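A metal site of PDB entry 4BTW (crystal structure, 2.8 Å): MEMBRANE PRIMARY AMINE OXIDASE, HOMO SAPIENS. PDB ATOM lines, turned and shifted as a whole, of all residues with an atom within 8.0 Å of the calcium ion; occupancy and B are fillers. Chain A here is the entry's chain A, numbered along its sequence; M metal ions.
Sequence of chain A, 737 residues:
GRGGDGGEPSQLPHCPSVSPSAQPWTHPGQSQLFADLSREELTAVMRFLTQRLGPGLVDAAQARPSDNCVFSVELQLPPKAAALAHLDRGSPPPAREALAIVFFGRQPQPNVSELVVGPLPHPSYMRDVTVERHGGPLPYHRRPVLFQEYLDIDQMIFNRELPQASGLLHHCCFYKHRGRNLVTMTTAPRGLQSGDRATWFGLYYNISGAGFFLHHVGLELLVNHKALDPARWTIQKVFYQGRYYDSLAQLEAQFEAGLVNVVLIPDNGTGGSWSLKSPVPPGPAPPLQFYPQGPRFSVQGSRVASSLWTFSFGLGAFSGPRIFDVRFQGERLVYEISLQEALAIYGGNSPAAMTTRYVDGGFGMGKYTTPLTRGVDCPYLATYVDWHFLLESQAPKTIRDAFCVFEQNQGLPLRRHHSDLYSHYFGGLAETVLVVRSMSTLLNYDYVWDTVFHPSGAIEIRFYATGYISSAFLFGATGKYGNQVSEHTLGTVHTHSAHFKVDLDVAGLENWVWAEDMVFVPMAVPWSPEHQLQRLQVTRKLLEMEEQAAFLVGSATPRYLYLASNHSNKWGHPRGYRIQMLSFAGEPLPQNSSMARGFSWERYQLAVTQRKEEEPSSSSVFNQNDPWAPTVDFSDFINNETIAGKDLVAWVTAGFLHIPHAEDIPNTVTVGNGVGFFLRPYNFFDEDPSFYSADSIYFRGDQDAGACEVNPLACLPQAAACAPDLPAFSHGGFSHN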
ATOM      1  N   LYS A  80     -23.456  -4.711   0.176  1.00  0.00           N
ATOM      2  CA  LYS A  80     -22.499  -5.101   1.192  1.00  0.00           C
ATOM      3  C   LYS A  80     -22.550  -4.174   2.405  1.00  0.00           C
ATOM      4  O   LYS A  80     -22.578  -4.647   3.541  1.00  0.00           O
ATOM      5  CB  LYS A  80     -21.094  -5.167   0.599  1.00  0.00           C
ATOM      6  CG  LYS A  80     -20.140  -6.005   1.428  1.00  0.00           C
ATOM      7  CD  LYS A  80     -18.768  -6.096   0.769  1.00  0.00           C
ATOM      8  CE  LYS A  80     -17.628  -6.123   1.778  1.00  0.00           C
ATOM      9  NZ  LYS A  80     -16.292  -6.193   1.153  1.00  0.00           N
ATOM     10  N   LEU A 333     -12.731 -13.251   7.840  1.00  0.00           N
ATOM     11  CA  LEU A 333     -11.680 -13.218   6.810  1.00  0.00           C
ATOM     12  C   LEU A 333     -12.125 -12.742   5.440  1.00  0.00           C
ATOM     13  O   LEU A 333     -11.494 -11.877   4.801  1.00  0.00           O
ATOM     14  CB  LEU A 333     -11.129 -14.604   6.632  1.00  0.00           C
ATOM     15  CG  LEU A 333     -10.551 -15.134   7.933  1.00  0.00           C
ATOM     16  CD1 LEU A 333     -10.340 -16.642   7.910  1.00  0.00           C
ATOM     17  CD2 LEU A 333      -9.229 -14.452   8.173  1.00  0.00           C
ATOM     18  N   VAL A 334     -13.209 -13.338   4.970  1.00  0.00           N
ATOM     19  CA  VAL A 334     -13.708 -13.040   3.627  1.00  0.00           C
ATOM     20  C   VAL A 334     -15.239 -12.905   3.624  1.00  0.00           C
ATOM     21  O   VAL A 334     -15.980 -13.672   4.283  1.00  0.00           O
ATOM     22  CB  VAL A 334     -13.179 -14.063   2.587  1.00  0.00           C
ATOM     23  CG1 VAL A 334     -12.959 -15.431   3.215  1.00  0.00           C
ATOM     24  CG2 VAL A 334     -14.104 -14.208   1.383  1.00  0.00           C
ATOM     25  N   TYR A 335     -15.669 -11.871   2.903  1.00  0.00           N
ATOM     26  CA  TYR A 335     -17.059 -11.555   2.805  1.00  0.00           C
ATOM     27  C   TYR A 335     -17.761 -12.605   1.909  1.00  0.00           C
ATOM     28  O   TYR A 335     -18.812 -13.127   2.286  1.00  0.00           O
ATOM     29  CB  TYR A 335     -17.239 -10.116   2.277  1.00  0.00           C
ATOM     30  CG  TYR A 335     -18.698  -9.782   1.971  1.00  0.00           C
ATOM     31  CD1 TYR A 335     -19.608  -9.563   2.987  1.00  0.00           C
ATOM     32  CD2 TYR A 335     -19.160  -9.726   0.666  1.00  0.00           C
ATOM     33  CE1 TYR A 335     -20.931  -9.251   2.710  1.00  0.00           C
ATOM     34  CE2 TYR A 335     -20.480  -9.420   0.382  1.00  0.00           C
ATOM     35  CZ  TYR A 335     -21.375  -9.187   1.409  1.00  0.00           C
ATOM     36  OH  TYR A 335     -22.720  -8.900   1.126  1.00  0.00           O
ATOM     37  N   VAL A 502     -12.899 -13.707  -4.981  1.00  0.00           N
ATOM     38  CA  VAL A 502     -12.431 -13.729  -3.606  1.00  0.00           C
ATOM     39  C   VAL A 502     -12.425 -12.282  -3.081  1.00  0.00           C
ATOM     40  O   VAL A 502     -11.545 -11.511  -3.434  1.00  0.00           O
ATOM     41  CB  VAL A 502     -11.043 -14.351  -3.534  1.00  0.00           C
ATOM     42  CG1 VAL A 502     -10.522 -14.415  -2.115  1.00  0.00           C
ATOM     43  CG2 VAL A 502     -11.119 -15.748  -4.090  1.00  0.00           C
ATOM     44  N   ASP A 503     -13.461 -11.953  -2.275  1.00  0.00           N
ATOM     45  CA  ASP A 503     -13.554 -10.661  -1.575  1.00  0.00           C
ATOM     46  C   ASP A 503     -13.072 -10.885  -0.189  1.00  0.00           C
ATOM     47  O   ASP A 503     -13.841 -11.061   0.752  1.00  0.00           O
ATOM     48  CB  ASP A 503     -14.992 -10.116  -1.506  1.00  0.00           C
ATOM     49  CG  ASP A 503     -15.067  -8.676  -0.934  1.00  0.00           C
ATOM     50  OD1 ASP A 503     -14.009  -8.008  -0.544  1.00  0.00           O
ATOM     51  OD2 ASP A 503     -16.248  -8.236  -0.903  1.00  0.00           O
ATOM     52  N   LEU A 504     -11.758 -10.889  -0.067  1.00  0.00           N
ATOM     53  CA  LEU A 504     -11.152 -10.745   1.210  1.00  0.00           C
ATOM     54  C   LEU A 504     -11.447  -9.363   1.730  1.00  0.00           C
ATOM     55  O   LEU A 504     -11.677  -8.383   1.000  1.00  0.00           O
ATOM     56  CB  LEU A 504      -9.652 -10.947   1.114  1.00  0.00           C
ATOM     57  CG  LEU A 504      -9.249 -12.413   1.085  1.00  0.00           C
ATOM     58  CD1 LEU A 504      -7.864 -12.619   0.493  1.00  0.00           C
ATOM     59  CD2 LEU A 504      -9.341 -12.987   2.495  1.00  0.00           C
ATOM     60  N   ASP A 505     -11.459  -9.335   3.048  1.00  0.00           N
ATOM     61  CA  ASP A 505     -11.664  -8.148   3.814  1.00  0.00           C
ATOM     62  C   ASP A 505     -10.857  -8.423   5.035  1.00  0.00           C
ATOM     63  O   ASP A 505     -11.385  -8.860   6.074  1.00  0.00           O
ATOM     64  CB  ASP A 505     -13.126  -8.018   4.157  1.00  0.00           C
ATOM     65  CG  ASP A 505     -13.944  -7.551   2.989  1.00  0.00           C
ATOM     66  OD1 ASP A 505     -13.362  -7.379   1.879  1.00  0.00           O
ATOM     67  OD2 ASP A 505     -15.170  -7.360   3.227  1.00  0.00           O
ATOM     68  N   VAL A 506      -9.552  -8.194   4.869  1.00  0.00           N
ATOM     69  CA  VAL A 506      -8.550  -8.645   5.833  1.00  0.00           C
ATOM     70  C   VAL A 506      -8.496  -7.729   7.037  1.00  0.00           C
ATOM     71  O   VAL A 506      -8.125  -6.556   6.899  1.00  0.00           O
ATOM     72  CB  VAL A 506      -7.142  -8.643   5.256  1.00  0.00           C
ATOM     73  CG1 VAL A 506      -6.254  -9.549   6.118  1.00  0.00           C
ATOM     74  CG2 VAL A 506      -7.169  -9.085   3.815  1.00  0.00           C
ATOM     75  N   GLY A 508     -10.648  -5.881   8.302  1.00  0.00           N
ATOM     76  CA  GLY A 508     -11.157  -4.647   7.755  1.00  0.00           C
ATOM     77  C   GLY A 508     -11.333  -4.640   6.252  1.00  0.00           C
ATOM     78  O   GLY A 508     -10.665  -5.335   5.516  1.00  0.00           O
ATOM     79  N   LEU A 509     -12.236  -3.801   5.796  1.00  0.00           N
ATOM     80  CA  LEU A 509     -12.418  -3.519   4.378  1.00  0.00           C
ATOM     81  C   LEU A 509     -11.218  -2.984   3.633  1.00  0.00           C
ATOM     82  O   LEU A 509     -10.982  -3.409   2.509  1.00  0.00           O
ATOM     83  CB  LEU A 509     -13.545  -2.485   4.177  1.00  0.00           C
ATOM     84  CG  LEU A 509     -14.828  -3.107   3.655  1.00  0.00           C
ATOM     85  CD1 LEU A 509     -15.404  -4.129   4.641  1.00  0.00           C
ATOM     86  CD2 LEU A 509     -15.799  -1.977   3.350  1.00  0.00           C
ATOM     87  N   GLU A 510     -10.524  -2.023   4.229  1.00  0.00           N
ATOM     88  CA  GLU A 510      -9.437  -1.316   3.543  1.00  0.00           C
ATOM     89  C   GLU A 510      -8.250  -2.262   3.518  1.00  0.00           C
ATOM     90  O   GLU A 510      -7.728  -2.652   4.579  1.00  0.00           O
ATOM     91  CB  GLU A 510      -9.071   0.017   4.208  1.00  0.00           C
ATOM     92  CG  GLU A 510     -10.219   1.004   4.408  1.00  0.00           C
ATOM     93  CD  GLU A 510     -11.176   0.634   5.551  1.00  0.00           C
ATOM     94  OE1 GLU A 510     -10.942  -0.360   6.294  1.00  0.00           O
ATOM     95  OE2 GLU A 510     -12.206   1.342   5.723  1.00  0.00           O
ATOM     96  N   ASN A 511      -7.885  -2.704   2.323  1.00  0.00           N
ATOM     97  CA  ASN A 511      -6.709  -3.528   2.148  1.00  0.00           C
ATOM     98  C   ASN A 511      -5.802  -2.908   1.088  1.00  0.00           C
ATOM     99  O   ASN A 511      -6.245  -2.131   0.232  1.00  0.00           O
ATOM    100  CB  ASN A 511      -7.066  -4.950   1.688  1.00  0.00           C
ATOM    101  CG  ASN A 511      -7.954  -5.709   2.659  1.00  0.00           C
ATOM    102  OD1 ASN A 511      -7.660  -5.799   3.880  1.00  0.00           O
ATOM    103  ND2 ASN A 511      -9.040  -6.315   2.101  1.00  0.00           N
ATOM    104  N   LEU A 563      -2.967  -9.987   0.136  1.00  0.00           N
ATOM    105  CA  LEU A 563      -3.662  -8.792   0.509  1.00  0.00           C
ATOM    106  C   LEU A 563      -3.556  -8.621   2.004  1.00  0.00           C
ATOM    107  O   LEU A 563      -3.631  -9.615   2.758  1.00  0.00           O
ATOM    108  CB  LEU A 563      -5.115  -8.897   0.132  1.00  0.00           C
ATOM    109  CG  LEU A 563      -5.515  -9.235  -1.301  1.00  0.00           C
ATOM    110  CD1 LEU A 563      -7.011  -8.995  -1.488  1.00  0.00           C
ATOM    111  CD2 LEU A 563      -4.728  -8.401  -2.298  1.00  0.00           C
ATOM    112  N   VAL A 608      -6.647  -7.984  -9.117  1.00  0.00           N
ATOM    113  CA  VAL A 608      -7.295  -7.387  -7.975  1.00  0.00           C
ATOM    114  C   VAL A 608      -7.871  -6.019  -8.334  1.00  0.00           C
ATOM    115  O   VAL A 608      -7.214  -5.167  -8.965  1.00  0.00           O
ATOM    116  CB  VAL A 608      -6.361  -7.315  -6.779  1.00  0.00           C
ATOM    117  CG1 VAL A 608      -7.145  -6.809  -5.594  1.00  0.00           C
ATOM    118  CG2 VAL A 608      -5.807  -8.689  -6.467  1.00  0.00           C
ATOM    119  N   THR A 609      -9.129  -5.835  -7.971  1.00  0.00           N
ATOM    120  CA  THR A 609      -9.833  -4.636  -8.333  1.00  0.00           C
ATOM    121  C   THR A 609     -10.488  -4.056  -7.115  1.00  0.00           C
ATOM    122  O   THR A 609     -10.619  -4.727  -6.054  1.00  0.00           O
ATOM    123  CB  THR A 609     -10.915  -4.928  -9.368  1.00  0.00           C
ATOM    124  OG1 THR A 609     -11.567  -6.149  -9.022  1.00  0.00           O
ATOM    125  CG2 THR A 609     -10.308  -5.089 -10.711  1.00  0.00           C
ATOM    126  N   GLN A 610     -10.875  -2.783  -7.282  1.00  0.00           N
ATOM    127  CA  GLN A 610     -11.824  -2.109  -6.399  1.00  0.00           C
ATOM    128  C   GLN A 610     -13.170  -2.796  -6.498  1.00  0.00           C
ATOM    129  O   GLN A 610     -13.755  -2.874  -7.613  1.00  0.00           O
ATOM    130  CB  GLN A 610     -12.008  -0.679  -6.828  1.00  0.00           C
ATOM    131  CG  GLN A 610     -11.091   0.275  -6.117  1.00  0.00           C
ATOM    132  CD  GLN A 610     -11.410   1.704  -6.463  1.00  0.00           C
ATOM    133  OE1 GLN A 610     -12.532   2.022  -6.835  1.00  0.00           O
ATOM    134  NE2 GLN A 610     -10.424   2.560  -6.332  1.00  0.00           N
ATOM    135  N   ARG A 611     -13.639  -3.271  -5.334  1.00  0.00           N
ATOM    136  CA  ARG A 611     -14.822  -4.119  -5.246  1.00  0.00           C
ATOM    137  C   ARG A 611     -16.009  -3.230  -5.395  1.00  0.00           C
ATOM    138  O   ARG A 611     -16.067  -2.200  -4.788  1.00  0.00           O
ATOM    139  CB  ARG A 611     -14.876  -4.864  -3.904  1.00  0.00           C
ATOM    140  CG  ARG A 611     -16.188  -5.592  -3.674  1.00  0.00           C
ATOM    141  CD  ARG A 611     -17.102  -4.766  -2.781  1.00  0.00           C
ATOM    142  NE  ARG A 611     -18.547  -4.927  -2.962  1.00  0.00           N
ATOM    143  CZ  ARG A 611     -19.235  -6.054  -2.745  1.00  0.00           C
ATOM    144  NH1 ARG A 611     -18.613  -7.201  -2.409  1.00  0.00           N
ATOM    145  NH2 ARG A 611     -20.555  -6.018  -2.906  1.00  0.00           N
ATOM    146  N   LYS A 646      -8.347  -0.254   0.141  1.00  0.00           N
ATOM    147  CA  LYS A 646      -9.762  -0.216  -0.283  1.00  0.00           C
ATOM    148  C   LYS A 646     -10.440  -1.562  -0.057  1.00  0.00           C
ATOM    149  O   LYS A 646      -9.808  -2.514   0.392  1.00  0.00           O
ATOM    150  CB  LYS A 646      -9.926   0.178  -1.750  1.00  0.00           C
ATOM    151  CG  LYS A 646      -8.973   1.245  -2.264  1.00  0.00           C
ATOM    152  CD  LYS A 646      -9.436   2.631  -1.908  1.00  0.00           C
ATOM    153  CE  LYS A 646     -10.553   3.077  -2.831  1.00  0.00           C
ATOM    154  NZ  LYS A 646     -10.534   4.548  -3.084  1.00  0.00           N
ATOM    155  N   ASP A 647     -11.742  -1.629  -0.387  1.00  0.00           N
ATOM    156  CA  ASP A 647     -12.438  -2.895  -0.419  1.00  0.00           C
ATOM    157  C   ASP A 647     -11.901  -3.658  -1.597  1.00  0.00           C
ATOM    158  O   ASP A 647     -11.994  -3.195  -2.772  1.00  0.00           O
ATOM    159  CB  ASP A 647     -13.944  -2.753  -0.576  1.00  0.00           C
ATOM    160  CG  ASP A 647     -14.696  -3.906   0.046  1.00  0.00           C
ATOM    161  OD1 ASP A 647     -14.057  -4.901   0.491  1.00  0.00           O
ATOM    162  OD2 ASP A 647     -15.930  -3.792   0.137  1.00  0.00           O
ATOM    163  N   LEU A 648     -11.332  -4.830  -1.336  1.00  0.00           N
ATOM    164  CA  LEU A 648     -10.536  -5.352  -2.435  1.00  0.00           C
ATOM    165  C   LEU A 648     -11.032  -6.708  -2.704  1.00  0.00           C
ATOM    166  O   LEU A 648     -11.290  -7.471  -1.758  1.00  0.00           O
ATOM    167  CB  LEU A 648      -9.037  -5.322  -2.142  1.00  0.00           C
ATOM    168  CG  LEU A 648      -8.302  -3.980  -2.311  1.00  0.00           C
ATOM    169  CD1 LEU A 648      -6.793  -4.195  -2.486  1.00  0.00           C
ATOM    170  CD2 LEU A 648      -8.842  -3.152  -3.468  1.00  0.00           C
ATOM    171  N   VAL A 649     -11.230  -6.966  -3.978  1.00  0.00           N
ATOM    172  CA  VAL A 649     -11.698  -8.259  -4.415  1.00  0.00           C
ATOM    173  C   VAL A 649     -10.723  -8.850  -5.442  1.00  0.00           C
ATOM    174  O   VAL A 649     -10.359  -8.239  -6.451  1.00  0.00           O
ATOM    175  CB  VAL A 649     -13.152  -8.201  -4.914  1.00  0.00           C
ATOM    176  CG1 VAL A 649     -13.262  -7.318  -6.145  1.00  0.00           C
ATOM    177  CG2 VAL A 649     -13.660  -9.609  -5.177  1.00  0.00           C
ATOM    178  N   ALA A 650     -10.247 -10.021  -5.092  1.00  0.00           N
ATOM    179  CA  ALA A 650      -9.303 -10.719  -5.893  1.00  0.00           C
ATOM    180  C   ALA A 650     -10.110 -11.613  -6.797  1.00  0.00           C
ATOM    181  O   ALA A 650     -11.197 -12.042  -6.426  1.00  0.00           O
ATOM    182  CB  ALA A 650      -8.393 -11.557  -5.004  1.00  0.00           C
HETATM  183 CA    CA M   1     -12.357  -6.406   0.037  1.00  0.00          CA
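The side-chain carboxylate (OD2) of Asp 503 lies within salt-bridge range of the side-chain amino group (NZ) of Lys 80, 2.9 Å away. O of Asp 647 lies within hydrogen-bond range of N of Arg 611 (3.0 Å). OD2 of Asp 647 is in salt-bridge range of NZ of Lys 80, 2.6 Å away. The side-chain amide oxygen (OD1) of Asn 511 lies close to the backbone carbonyl oxygen (O) of Val 506. O of Leu 509 sits close to N of Asp 647. O of Asp 503 lies within hydrogen-bond range of N of Tyr 335. The side-chain carboxylate of Asp 503 lies within salt-bridge range of the guanidinium group of Arg 611. The backbone NH (N) of Asn 511 is in hydrogen-bond range of the backbone carbonyl oxygen (O) of Lys 646.
Merely in contact with the calcium ion: Asn 511 (3.9 Å).
O of Leu 504 binds the calcium ion (2.3 Å). OD1 of Asp 505 binds the calcium ion, 2.3 Å away. The calcium ion is bound by the side-chain carboxylate (OD1) of Asp 647 (2.3 Å). The calcium ion is bound by the backbone nitrogen (N) of Leu 648, at 2.3 Å. The calcium ion is bound by O of Leu 648 (2.3 Å). OD1 of Asp 503 binds the calcium ion.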
